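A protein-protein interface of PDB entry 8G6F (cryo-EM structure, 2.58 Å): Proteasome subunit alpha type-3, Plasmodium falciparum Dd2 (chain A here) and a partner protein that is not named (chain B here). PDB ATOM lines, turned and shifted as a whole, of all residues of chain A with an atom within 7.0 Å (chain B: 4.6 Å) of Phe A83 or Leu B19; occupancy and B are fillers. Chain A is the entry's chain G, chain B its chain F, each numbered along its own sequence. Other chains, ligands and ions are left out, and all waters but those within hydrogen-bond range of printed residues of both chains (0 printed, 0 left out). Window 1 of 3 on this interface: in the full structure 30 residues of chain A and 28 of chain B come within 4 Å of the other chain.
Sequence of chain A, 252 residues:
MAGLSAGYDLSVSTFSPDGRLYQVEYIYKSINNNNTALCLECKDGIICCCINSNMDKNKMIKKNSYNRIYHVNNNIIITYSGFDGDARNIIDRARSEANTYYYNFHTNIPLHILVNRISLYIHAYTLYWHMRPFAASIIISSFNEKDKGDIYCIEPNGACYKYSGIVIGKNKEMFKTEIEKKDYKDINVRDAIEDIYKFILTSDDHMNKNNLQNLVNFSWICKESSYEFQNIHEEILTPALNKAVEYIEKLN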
ATOM      1  N   GLN A  23     -27.280  10.402  15.132  1.00  0.00           N
ATOM      2  CA  GLN A  23     -26.423   9.703  14.184  1.00  0.00           C
ATOM      3  C   GLN A  23     -25.326  10.621  13.669  1.00  0.00           C
ATOM      4  O   GLN A  23     -24.161  10.219  13.568  1.00  0.00           O
ATOM      5  CB  GLN A  23     -27.255   9.156  13.028  1.00  0.00           C
ATOM      6  CG  GLN A  23     -28.010   7.884  13.358  1.00  0.00           C
ATOM      7  CD  GLN A  23     -27.095   6.702  13.573  1.00  0.00           C
ATOM      8  OE1 GLN A  23     -26.631   6.088  12.619  1.00  0.00           O
ATOM      9  NE2 GLN A  23     -26.837   6.372  14.829  1.00  0.00           N
ATOM     10  N   SER A  30     -16.773   9.928  15.573  1.00  0.00           N
ATOM     11  CA  SER A  30     -15.892   9.096  14.761  1.00  0.00           C
ATOM     12  C   SER A  30     -14.821   9.934  14.080  1.00  0.00           C
ATOM     13  O   SER A  30     -13.644   9.560  14.064  1.00  0.00           O
ATOM     14  CB  SER A  30     -16.708   8.333  13.721  1.00  0.00           C
ATOM     15  OG  SER A  30     -15.875   7.819  12.702  1.00  0.00           O
ATOM     16  N   ILE A  31     -15.211  11.072  13.507  1.00  0.00           N
ATOM     17  CA  ILE A  31     -14.243  11.921  12.820  1.00  0.00           C
ATOM     18  C   ILE A  31     -13.227  12.479  13.805  1.00  0.00           C
ATOM     19  O   ILE A  31     -12.026  12.526  13.519  1.00  0.00           O
ATOM     20  CB  ILE A  31     -14.963  13.046  12.059  1.00  0.00           C
ATOM     21  CG1 ILE A  31     -15.749  12.463  10.889  1.00  0.00           C
ATOM     22  CG2 ILE A  31     -13.963  14.069  11.557  1.00  0.00           C
ATOM     23  CD1 ILE A  31     -16.776  13.401  10.345  1.00  0.00           C
ATOM     24  N   ASN A  34     -10.221  10.332  14.541  1.00  0.00           N
ATOM     25  CA  ASN A  34      -9.425   9.896  13.405  1.00  0.00           C
ATOM     26  C   ASN A  34      -8.147  10.728  13.283  1.00  0.00           C
ATOM     27  O   ASN A  34      -7.818  11.539  14.151  1.00  0.00           O
ATOM     28  CB  ASN A  34     -10.268   9.967  12.132  1.00  0.00           C
ATOM     29  CG  ASN A  34     -10.207   8.688  11.323  1.00  0.00           C
ATOM     30  OD1 ASN A  34      -9.137   8.129  11.103  1.00  0.00           O
ATOM     31  ND2 ASN A  34     -11.364   8.212  10.885  1.00  0.00           N
ATOM     32  N   TYR A  66       0.724   6.082   1.899  1.00  0.00           N
ATOM     33  CA  TYR A  66      -0.600   6.499   2.343  1.00  0.00           C
ATOM     34  C   TYR A  66      -0.665   8.022   2.340  1.00  0.00           C
ATOM     35  O   TYR A  66       0.029   8.683   3.117  1.00  0.00           O
ATOM     36  CB  TYR A  66      -0.904   5.940   3.728  1.00  0.00           C
ATOM     37  CG  TYR A  66      -2.276   6.302   4.230  1.00  0.00           C
ATOM     38  CD1 TYR A  66      -3.413   5.814   3.610  1.00  0.00           C
ATOM     39  CD2 TYR A  66      -2.436   7.132   5.324  1.00  0.00           C
ATOM     40  CE1 TYR A  66      -4.666   6.143   4.066  1.00  0.00           C
ATOM     41  CE2 TYR A  66      -3.685   7.467   5.785  1.00  0.00           C
ATOM     42  CZ  TYR A  66      -4.796   6.970   5.154  1.00  0.00           C
ATOM     43  OH  TYR A  66      -6.045   7.305   5.618  1.00  0.00           O
ATOM     44  N   TYR A  80      -9.053  15.304   3.902  1.00  0.00           N
ATOM     45  CA  TYR A  80     -10.189  14.807   4.659  1.00  0.00           C
ATOM     46  C   TYR A  80      -9.723  14.207   5.971  1.00  0.00           C
ATOM     47  O   TYR A  80      -8.540  13.931   6.177  1.00  0.00           O
ATOM     48  CB  TYR A  80     -10.973  13.764   3.864  1.00  0.00           C
ATOM     49  CG  TYR A  80     -10.232  12.465   3.664  1.00  0.00           C
ATOM     50  CD1 TYR A  80     -10.301  11.450   4.605  1.00  0.00           C
ATOM     51  CD2 TYR A  80      -9.476  12.244   2.524  1.00  0.00           C
ATOM     52  CE1 TYR A  80      -9.633  10.264   4.422  1.00  0.00           C
ATOM     53  CE2 TYR A  80      -8.810  11.060   2.333  1.00  0.00           C
ATOM     54  CZ  TYR A  80      -8.890  10.076   3.284  1.00  0.00           C
ATOM     55  OH  TYR A  80      -8.223   8.894   3.095  1.00  0.00           O
ATOM     56  N   SER A  81     -10.690  14.011   6.861  1.00  0.00           N
ATOM     57  CA  SER A  81     -10.492  13.275   8.102  1.00  0.00           C
ATOM     58  C   SER A  81     -11.724  12.415   8.328  1.00  0.00           C
ATOM     59  O   SER A  81     -12.830  12.945   8.458  1.00  0.00           O
ATOM     60  CB  SER A  81     -10.265  14.224   9.279  1.00  0.00           C
ATOM     61  OG  SER A  81      -9.409  13.639  10.238  1.00  0.00           O
ATOM     62  N   GLY A  82     -11.544  11.110   8.350  1.00  0.00           N
ATOM     63  CA  GLY A  82     -12.657  10.190   8.480  1.00  0.00           C
ATOM     64  C   GLY A  82     -12.362   8.891   7.746  1.00  0.00           C
ATOM     65  O   GLY A  82     -11.215   8.468   7.653  1.00  0.00           O
ATOM     66  N   PHE A  83     -13.425   8.275   7.235  1.00  0.00           N
ATOM     67  CA  PHE A  83     -13.308   6.999   6.543  1.00  0.00           C
ATOM     68  C   PHE A  83     -12.710   7.195   5.157  1.00  0.00           C
ATOM     69  O   PHE A  83     -13.147   8.065   4.396  1.00  0.00           O
ATOM     70  CB  PHE A  83     -14.674   6.325   6.429  1.00  0.00           C
ATOM     71  CG  PHE A  83     -15.238   5.849   7.739  1.00  0.00           C
ATOM     72  CD1 PHE A  83     -14.468   5.825   8.887  1.00  0.00           C
ATOM     73  CD2 PHE A  83     -16.546   5.416   7.815  1.00  0.00           C
ATOM     74  CE1 PHE A  83     -14.994   5.385  10.078  1.00  0.00           C
ATOM     75  CE2 PHE A  83     -17.076   4.975   9.005  1.00  0.00           C
ATOM     76  CZ  PHE A  83     -16.299   4.960  10.136  1.00  0.00           C
ATOM     77  N   ASP A  84     -11.717   6.366   4.829  1.00  0.00           N
ATOM     78  CA  ASP A  84     -11.034   6.494   3.548  1.00  0.00           C
ATOM     79  C   ASP A  84     -11.993   6.289   2.388  1.00  0.00           C
ATOM     80  O   ASP A  84     -11.951   7.030   1.404  1.00  0.00           O
ATOM     81  CB  ASP A  84      -9.889   5.489   3.464  1.00  0.00           C
ATOM     82  CG  ASP A  84      -8.772   5.800   4.427  1.00  0.00           C
ATOM     83  OD1 ASP A  84      -8.266   6.937   4.403  1.00  0.00           O
ATOM     84  OD2 ASP A  84      -8.396   4.906   5.209  1.00  0.00           O
ATOM     85  N   GLY A  85     -12.865   5.287   2.485  1.00  0.00           N
ATOM     86  CA  GLY A  85     -13.791   5.024   1.399  1.00  0.00           C
ATOM     87  C   GLY A  85     -14.771   6.159   1.176  1.00  0.00           C
ATOM     88  O   GLY A  85     -15.009   6.578   0.040  1.00  0.00           O
ATOM     89  N   ASP A  86     -15.358   6.671   2.259  1.00  0.00           N
ATOM     90  CA  ASP A  86     -16.300   7.778   2.136  1.00  0.00           C
ATOM     91  C   ASP A  86     -15.622   9.015   1.572  1.00  0.00           C
ATOM     92  O   ASP A  86     -16.171   9.695   0.695  1.00  0.00           O
ATOM     93  CB  ASP A  86     -16.918   8.090   3.499  1.00  0.00           C
ATOM     94  CG  ASP A  86     -17.886   7.030   3.953  1.00  0.00           C
ATOM     95  OD1 ASP A  86     -18.175   6.113   3.160  1.00  0.00           O
ATOM     96  OD2 ASP A  86     -18.363   7.110   5.101  1.00  0.00           O
ATOM     97  N   ALA A  87     -14.423   9.324   2.063  1.00  0.00           N
ATOM     98  CA  ALA A  87     -13.697  10.475   1.549  1.00  0.00           C
ATOM     99  C   ALA A  87     -13.359  10.302   0.077  1.00  0.00           C
ATOM    100  O   ALA A  87     -13.436  11.258  -0.698  1.00  0.00           O
ATOM    101  CB  ALA A  87     -12.428  10.689   2.355  1.00  0.00           C
ATOM    102  N   ARG A  88     -12.960   9.096  -0.323  1.00  0.00           N
ATOM    103  CA  ARG A  88     -12.668   8.843  -1.726  1.00  0.00           C
ATOM    104  C   ARG A  88     -13.910   9.045  -2.580  1.00  0.00           C
ATOM    105  O   ARG A  88     -13.837   9.617  -3.671  1.00  0.00           O
ATOM    106  CB  ARG A  88     -12.128   7.425  -1.884  1.00  0.00           C
ATOM    107  CG  ARG A  88     -11.125   7.248  -3.000  1.00  0.00           C
ATOM    108  CD  ARG A  88     -10.435   5.901  -2.900  1.00  0.00           C
ATOM    109  NE  ARG A  88     -11.386   4.835  -2.608  1.00  0.00           N
ATOM    110  CZ  ARG A  88     -11.371   4.069  -1.525  1.00  0.00           C
ATOM    111  NH1 ARG A  88     -10.430   4.183  -0.603  1.00  0.00           N
ATOM    112  NH2 ARG A  88     -12.332   3.168  -1.359  1.00  0.00           N
ATOM    113  N   ASN A  89     -15.058   8.583  -2.092  1.00  0.00           N
ATOM    114  CA  ASN A  89     -16.319   8.799  -2.790  1.00  0.00           C
ATOM    115  C   ASN A  89     -16.597  10.287  -2.973  1.00  0.00           C
ATOM    116  O   ASN A  89     -16.974  10.740  -4.063  1.00  0.00           O
ATOM    117  CB  ASN A  89     -17.440   8.129  -1.996  1.00  0.00           C
ATOM    118  CG  ASN A  89     -18.679   7.892  -2.815  1.00  0.00           C
ATOM    119  OD1 ASN A  89     -19.616   8.686  -2.785  1.00  0.00           O
ATOM    120  ND2 ASN A  89     -18.702   6.789  -3.547  1.00  0.00           N
ATOM    121  N   ARG A 132     -26.453   5.382   4.553  1.00  0.00           N
ATOM    122  CA  ARG A 132     -25.519   5.689   5.624  1.00  0.00           C
ATOM    123  C   ARG A 132     -24.857   7.028   5.353  1.00  0.00           C
ATOM    124  O   ARG A 132     -24.253   7.196   4.282  1.00  0.00           O
ATOM    125  CB  ARG A 132     -24.460   4.600   5.742  1.00  0.00           C
ATOM    126  CG  ARG A 132     -23.446   4.854   6.838  1.00  0.00           C
ATOM    127  CD  ARG A 132     -22.453   3.722   6.959  1.00  0.00           C
ATOM    128  NE  ARG A 132     -21.619   3.585   5.773  1.00  0.00           N
ATOM    129  CZ  ARG A 132     -20.523   4.290   5.536  1.00  0.00           C
ATOM    130  NH1 ARG A 132     -20.098   5.215   6.379  1.00  0.00           N
ATOM    131  NH2 ARG A 132     -19.837   4.065   4.421  1.00  0.00           N
ATOM    132  N   PRO A 133     -24.933   8.000   6.261  1.00  0.00           N
ATOM    133  CA  PRO A 133     -24.239   9.271   6.032  1.00  0.00           C
ATOM    134  C   PRO A 133     -22.728   9.096   5.960  1.00  0.00           C
ATOM    135  O   PRO A 133     -22.154   8.186   6.558  1.00  0.00           O
ATOM    136  CB  PRO A 133     -24.641  10.117   7.242  1.00  0.00           C
ATOM    137  CG  PRO A 133     -25.853   9.489   7.776  1.00  0.00           C
ATOM    138  CD  PRO A 133     -25.754   8.039   7.481  1.00  0.00           C
ATOM    139  N   PHE A 134     -22.086   9.992   5.212  1.00  0.00           N
ATOM    140  CA  PHE A 134     -20.633   9.987   5.102  1.00  0.00           C
ATOM    141  C   PHE A 134     -19.999  10.382   6.428  1.00  0.00           C
ATOM    142  O   PHE A 134     -20.372  11.392   7.030  1.00  0.00           O
ATOM    143  CB  PHE A 134     -20.178  10.955   4.014  1.00  0.00           C
ATOM    144  CG  PHE A 134     -20.621  10.576   2.637  1.00  0.00           C
ATOM    145  CD1 PHE A 134     -20.100   9.463   2.010  1.00  0.00           C
ATOM    146  CD2 PHE A 134     -21.551  11.341   1.963  1.00  0.00           C
ATOM    147  CE1 PHE A 134     -20.503   9.118   0.744  1.00  0.00           C
ATOM    148  CE2 PHE A 134     -21.955  11.000   0.698  1.00  0.00           C
ATOM    149  CZ  PHE A 134     -21.431   9.885   0.088  1.00  0.00           C
ATOM    150  N   ALA A 135     -19.031   9.586   6.880  1.00  0.00           N
ATOM    151  CA  ALA A 135     -18.282   9.882   8.098  1.00  0.00           C
ATOM    152  C   ALA A 135     -16.934  10.475   7.703  1.00  0.00           C
ATOM    153  O   ALA A 135     -15.897   9.816   7.737  1.00  0.00           O
ATOM    154  CB  ALA A 135     -18.123   8.629   8.948  1.00  0.00           C
ATOM    155  N   ALA A 136     -16.954  11.751   7.328  1.00  0.00           N
ATOM    156  CA  ALA A 136     -15.738  12.428   6.909  1.00  0.00           C
ATOM    157  C   ALA A 136     -15.951  13.932   6.958  1.00  0.00           C
ATOM    158  O   ALA A 136     -17.029  14.421   6.616  1.00  0.00           O
ATOM    159  CB  ALA A 136     -15.323  12.001   5.498  1.00  0.00           C
ATOM    160  N   SER A 137     -14.921  14.650   7.390  1.00  0.00           N
ATOM    161  CA  SER A 137     -14.863  16.102   7.301  1.00  0.00           C
ATOM    162  C   SER A 137     -13.879  16.476   6.206  1.00  0.00           C
ATOM    163  O   SER A 137     -12.758  15.964   6.177  1.00  0.00           O
ATOM    164  CB  SER A 137     -14.440  16.728   8.628  1.00  0.00           C
ATOM    165  OG  SER A 137     -15.565  17.091   9.401  1.00  0.00           O
ATOM    166  N   ASN B  10     -26.180  -2.153   8.917  1.00  0.00           N
ATOM    167  CA  ASN B  10     -24.877  -1.657   8.502  1.00  0.00           C
ATOM    168  C   ASN B  10     -24.847  -0.159   8.241  1.00  0.00           C
ATOM    169  O   ASN B  10     -23.804   0.357   7.830  1.00  0.00           O
ATOM    170  CB  ASN B  10     -24.412  -2.400   7.247  1.00  0.00           C
ATOM    171  CG  ASN B  10     -25.342  -2.198   6.074  1.00  0.00           C
ATOM    172  OD1 ASN B  10     -26.540  -1.989   6.248  1.00  0.00           O
ATOM    173  ND2 ASN B  10     -24.795  -2.263   4.867  1.00  0.00           N
ATOM    174  N   ILE B  12     -25.941   2.102  10.680  1.00  0.00           N
ATOM    175  CA  ILE B  12     -26.121   2.713  11.990  1.00  0.00           C
ATOM    176  C   ILE B  12     -24.763   2.816  12.664  1.00  0.00           C
ATOM    177  O   ILE B  12     -24.045   1.817  12.783  1.00  0.00           O
ATOM    178  CB  ILE B  12     -27.103   1.906  12.858  1.00  0.00           C
ATOM    179  CG1 ILE B  12     -28.466   1.827  12.176  1.00  0.00           C
ATOM    180  CG2 ILE B  12     -27.237   2.531  14.235  1.00  0.00           C
ATOM    181  CD1 ILE B  12     -29.402   0.831  12.807  1.00  0.00           C
ATOM    182  N   TYR B  13     -24.415   4.019  13.106  1.00  0.00           N
ATOM    183  CA  TYR B  13     -23.222   4.235  13.904  1.00  0.00           C
ATOM    184  C   TYR B  13     -23.549   4.022  15.373  1.00  0.00           C
ATOM    185  O   TYR B  13     -24.625   4.396  15.842  1.00  0.00           O
ATOM    186  CB  TYR B  13     -22.673   5.648  13.701  1.00  0.00           C
ATOM    187  CG  TYR B  13     -22.270   5.962  12.281  1.00  0.00           C
ATOM    188  CD1 TYR B  13     -23.210   6.361  11.348  1.00  0.00           C
ATOM    189  CD2 TYR B  13     -20.945   5.871  11.878  1.00  0.00           C
ATOM    190  CE1 TYR B  13     -22.852   6.650  10.055  1.00  0.00           C
ATOM    191  CE2 TYR B  13     -20.576   6.161  10.586  1.00  0.00           C
ATOM    192  CZ  TYR B  13     -21.535   6.550   9.678  1.00  0.00           C
ATOM    193  OH  TYR B  13     -21.180   6.841   8.384  1.00  0.00           O
ATOM    194  N   GLY B  17     -19.370   6.008  17.178  1.00  0.00           N
ATOM    195  CA  GLY B  17     -19.116   6.192  15.761  1.00  0.00           C
ATOM    196  C   GLY B  17     -18.513   4.987  15.075  1.00  0.00           C
ATOM    197  O   GLY B  17     -17.602   5.140  14.254  1.00  0.00           O
ATOM    198  N   ARG B  18     -19.008   3.791  15.378  1.00  0.00           N
ATOM    199  CA  ARG B  18     -18.483   2.556  14.820  1.00  0.00           C
ATOM    200  C   ARG B  18     -19.551   1.854  13.994  1.00  0.00           C
ATOM    201  O   ARG B  18     -20.746   1.960  14.275  1.00  0.00           O
ATOM    202  CB  ARG B  18     -17.992   1.625  15.926  1.00  0.00           C
ATOM    203  CG  ARG B  18     -16.708   2.082  16.583  1.00  0.00           C
ATOM    204  CD  ARG B  18     -16.434   1.306  17.850  1.00  0.00           C
ATOM    205  NE  ARG B  18     -16.282  -0.120  17.592  1.00  0.00           N
ATOM    206  CZ  ARG B  18     -15.796  -0.992  18.464  1.00  0.00           C
ATOM    207  NH1 ARG B  18     -15.398  -0.616  19.668  1.00  0.00           N
ATOM    208  NH2 ARG B  18     -15.709  -2.273  18.121  1.00  0.00           N
ATOM    209  N   LEU B  19     -19.105   1.135  12.966  1.00  0.00           N
ATOM    210  CA  LEU B  19     -19.978   0.366  12.082  1.00  0.00           C
ATOM    211  C   LEU B  19     -19.745  -1.111  12.383  1.00  0.00           C
ATOM    212  O   LEU B  19     -18.860  -1.749  11.810  1.00  0.00           O
ATOM    213  CB  LEU B  19     -19.711   0.692  10.620  1.00  0.00           C
ATOM    214  CG  LEU B  19     -20.001   2.128  10.182  1.00  0.00           C
ATOM    215  CD1 LEU B  19     -19.493   2.361   8.777  1.00  0.00           C
ATOM    216  CD2 LEU B  19     -21.486   2.424  10.265  1.00  0.00           C
ATOM    217  N   TYR B  20     -20.565  -1.653  13.283  1.00  0.00           N
ATOM    218  CA  TYR B  20     -20.333  -3.002  13.781  1.00  0.00           C
ATOM    219  C   TYR B  20     -20.488  -4.049  12.691  1.00  0.00           C
ATOM    220  O   TYR B  20     -19.781  -5.059  12.708  1.00  0.00           O
ATOM    221  CB  TYR B  20     -21.279  -3.299  14.939  1.00  0.00           C
ATOM    222  CG  TYR B  20     -20.835  -2.697  16.249  1.00  0.00           C
ATOM    223  CD1 TYR B  20     -19.599  -3.006  16.792  1.00  0.00           C
ATOM    224  CD2 TYR B  20     -21.652  -1.821  16.942  1.00  0.00           C
ATOM    225  CE1 TYR B  20     -19.191  -2.460  17.984  1.00  0.00           C
ATOM    226  CE2 TYR B  20     -21.250  -1.271  18.136  1.00  0.00           C
ATOM    227  CZ  TYR B  20     -20.018  -1.593  18.652  1.00  0.00           C
ATOM    228  OH  TYR B  20     -19.610  -1.047  19.843  1.00  0.00           O
ATOM    229  N   GLN B  21     -21.405  -3.851  11.748  1.00  0.00           N
ATOM    230  CA  GLN B  21     -21.558  -4.824  10.673  1.00  0.00           C
ATOM    231  C   GLN B  21     -20.296  -4.906   9.823  1.00  0.00           C
ATOM    232  O   GLN B  21     -19.852  -6.000   9.456  1.00  0.00           O
ATOM    233  CB  GLN B  21     -22.768  -4.465   9.816  1.00  0.00           C
ATOM    234  CG  GLN B  21     -24.091  -4.828  10.457  1.00  0.00           C
ATOM    235  CD  GLN B  21     -24.303  -6.321  10.538  1.00  0.00           C
ATOM    236  OE1 GLN B  21     -24.381  -6.999   9.519  1.00  0.00           O
ATOM    237  NE2 GLN B  21     -24.392  -6.843  11.753  1.00  0.00           N
ATOM    238  N   VAL B  22     -19.702  -3.756   9.506  1.00  0.00           N
ATOM    239  CA  VAL B  22     -18.446  -3.748   8.765  1.00  0.00           C
ATOM    240  C   VAL B  22     -17.338  -4.376   9.600  1.00  0.00           C
ATOM    241  O   VAL B  22     -16.483  -5.106   9.080  1.00  0.00           O
ATOM    242  CB  VAL B  22     -18.099  -2.311   8.337  1.00  0.00           C
ATOM    243  CG1 VAL B  22     -16.869  -2.299   7.458  1.00  0.00           C
ATOM    244  CG2 VAL B  22     -19.273  -1.682   7.611  1.00  0.00           C
ATOM    245  N   GLU B  23     -17.337  -4.113  10.907  1.00  0.00           N
ATOM    246  CA  GLU B  23     -16.336  -4.728  11.772  1.00  0.00           C
ATOM    247  C   GLU B  23     -16.470  -6.246  11.779  1.00  0.00           C
ATOM    248  O   GLU B  23     -15.471  -6.963  11.858  1.00  0.00           O
ATOM    249  CB  GLU B  23     -16.459  -4.174  13.188  1.00  0.00           C
ATOM    250  CG  GLU B  23     -16.080  -2.715  13.310  1.00  0.00           C
ATOM    251  CD  GLU B  23     -16.005  -2.263  14.747  1.00  0.00           C
ATOM    252  OE1 GLU B  23     -16.446  -3.025  15.630  1.00  0.00           O
ATOM    253  OE2 GLU B  23     -15.504  -1.148  14.999  1.00  0.00           O
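Among the printed residues, pairs that only touch across the chains: Gln A23 with Ile B12 (3.5 Å), Ser A30 with Gly B17 (3.4 Å), Phe A83 with Leu B19 (3.6 Å), Arg A132 with Asn B10 (3.7 Å), Arg A132 with Leu B19 (3.7 Å) and Ala A135 with Tyr B13 (3.6 Å).
Hydrophobic or aromatic side chains of chain A within 4 Å of the printed part of chain B: Phe A83 and Ala A135.
Hydrophobic or aromatic side chains of chain B that line the printed part of chain A: Ile B12, Tyr B13 and Leu B19.
The side-chain hydroxyl (OH) of Tyr B13 sits at hydrogen-bond distance from the guanidinium group (NH1) of Arg A132 (2.8 Å).
OH of Tyr B13 sits at hydrogen-bond distance from O of Pro A133.
N of Tyr B13 is in hydrogen-bond range of OE1 of Gln A23, at 3.1 Å.
Printed residues of chain B within 4 Å of Ser A30: Gly B17 (3.4 Å).
Tyr A80 touches none of the printed residues of chain B.
Of the printed residues of chain B, Arg A132 touches Asn B10 (3.7 Å), Tyr B13 (2.8 Å) and Leu B19 (3.7 Å).
Printed residues of chain A within 4 Å of Asn B10: Arg A132 (3.7 Å).
Of the printed residues of chain A, Tyr B13 touches Gln A23 (3.1 Å), Arg A132 (2.8 Å), Pro A133 (2.5 Å) and Ala A135 (3.6 Å).
Printed residues of chain A within 4 Å of Gly B17: Ser A30 (3.4 Å).
The nearest printed residue of chain B that does not touch Phe A83 is Tyr B13 (4.02 Å).
OD2 of Asp A86 sits at hydrogen-bond distance from N of Ala A135.
N of Phe A83 lies within hydrogen-bond range of O of Ala A135.
OD2 of Asp A86 is in salt-bridge range of NH1 of Arg A132 (2.9 Å).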
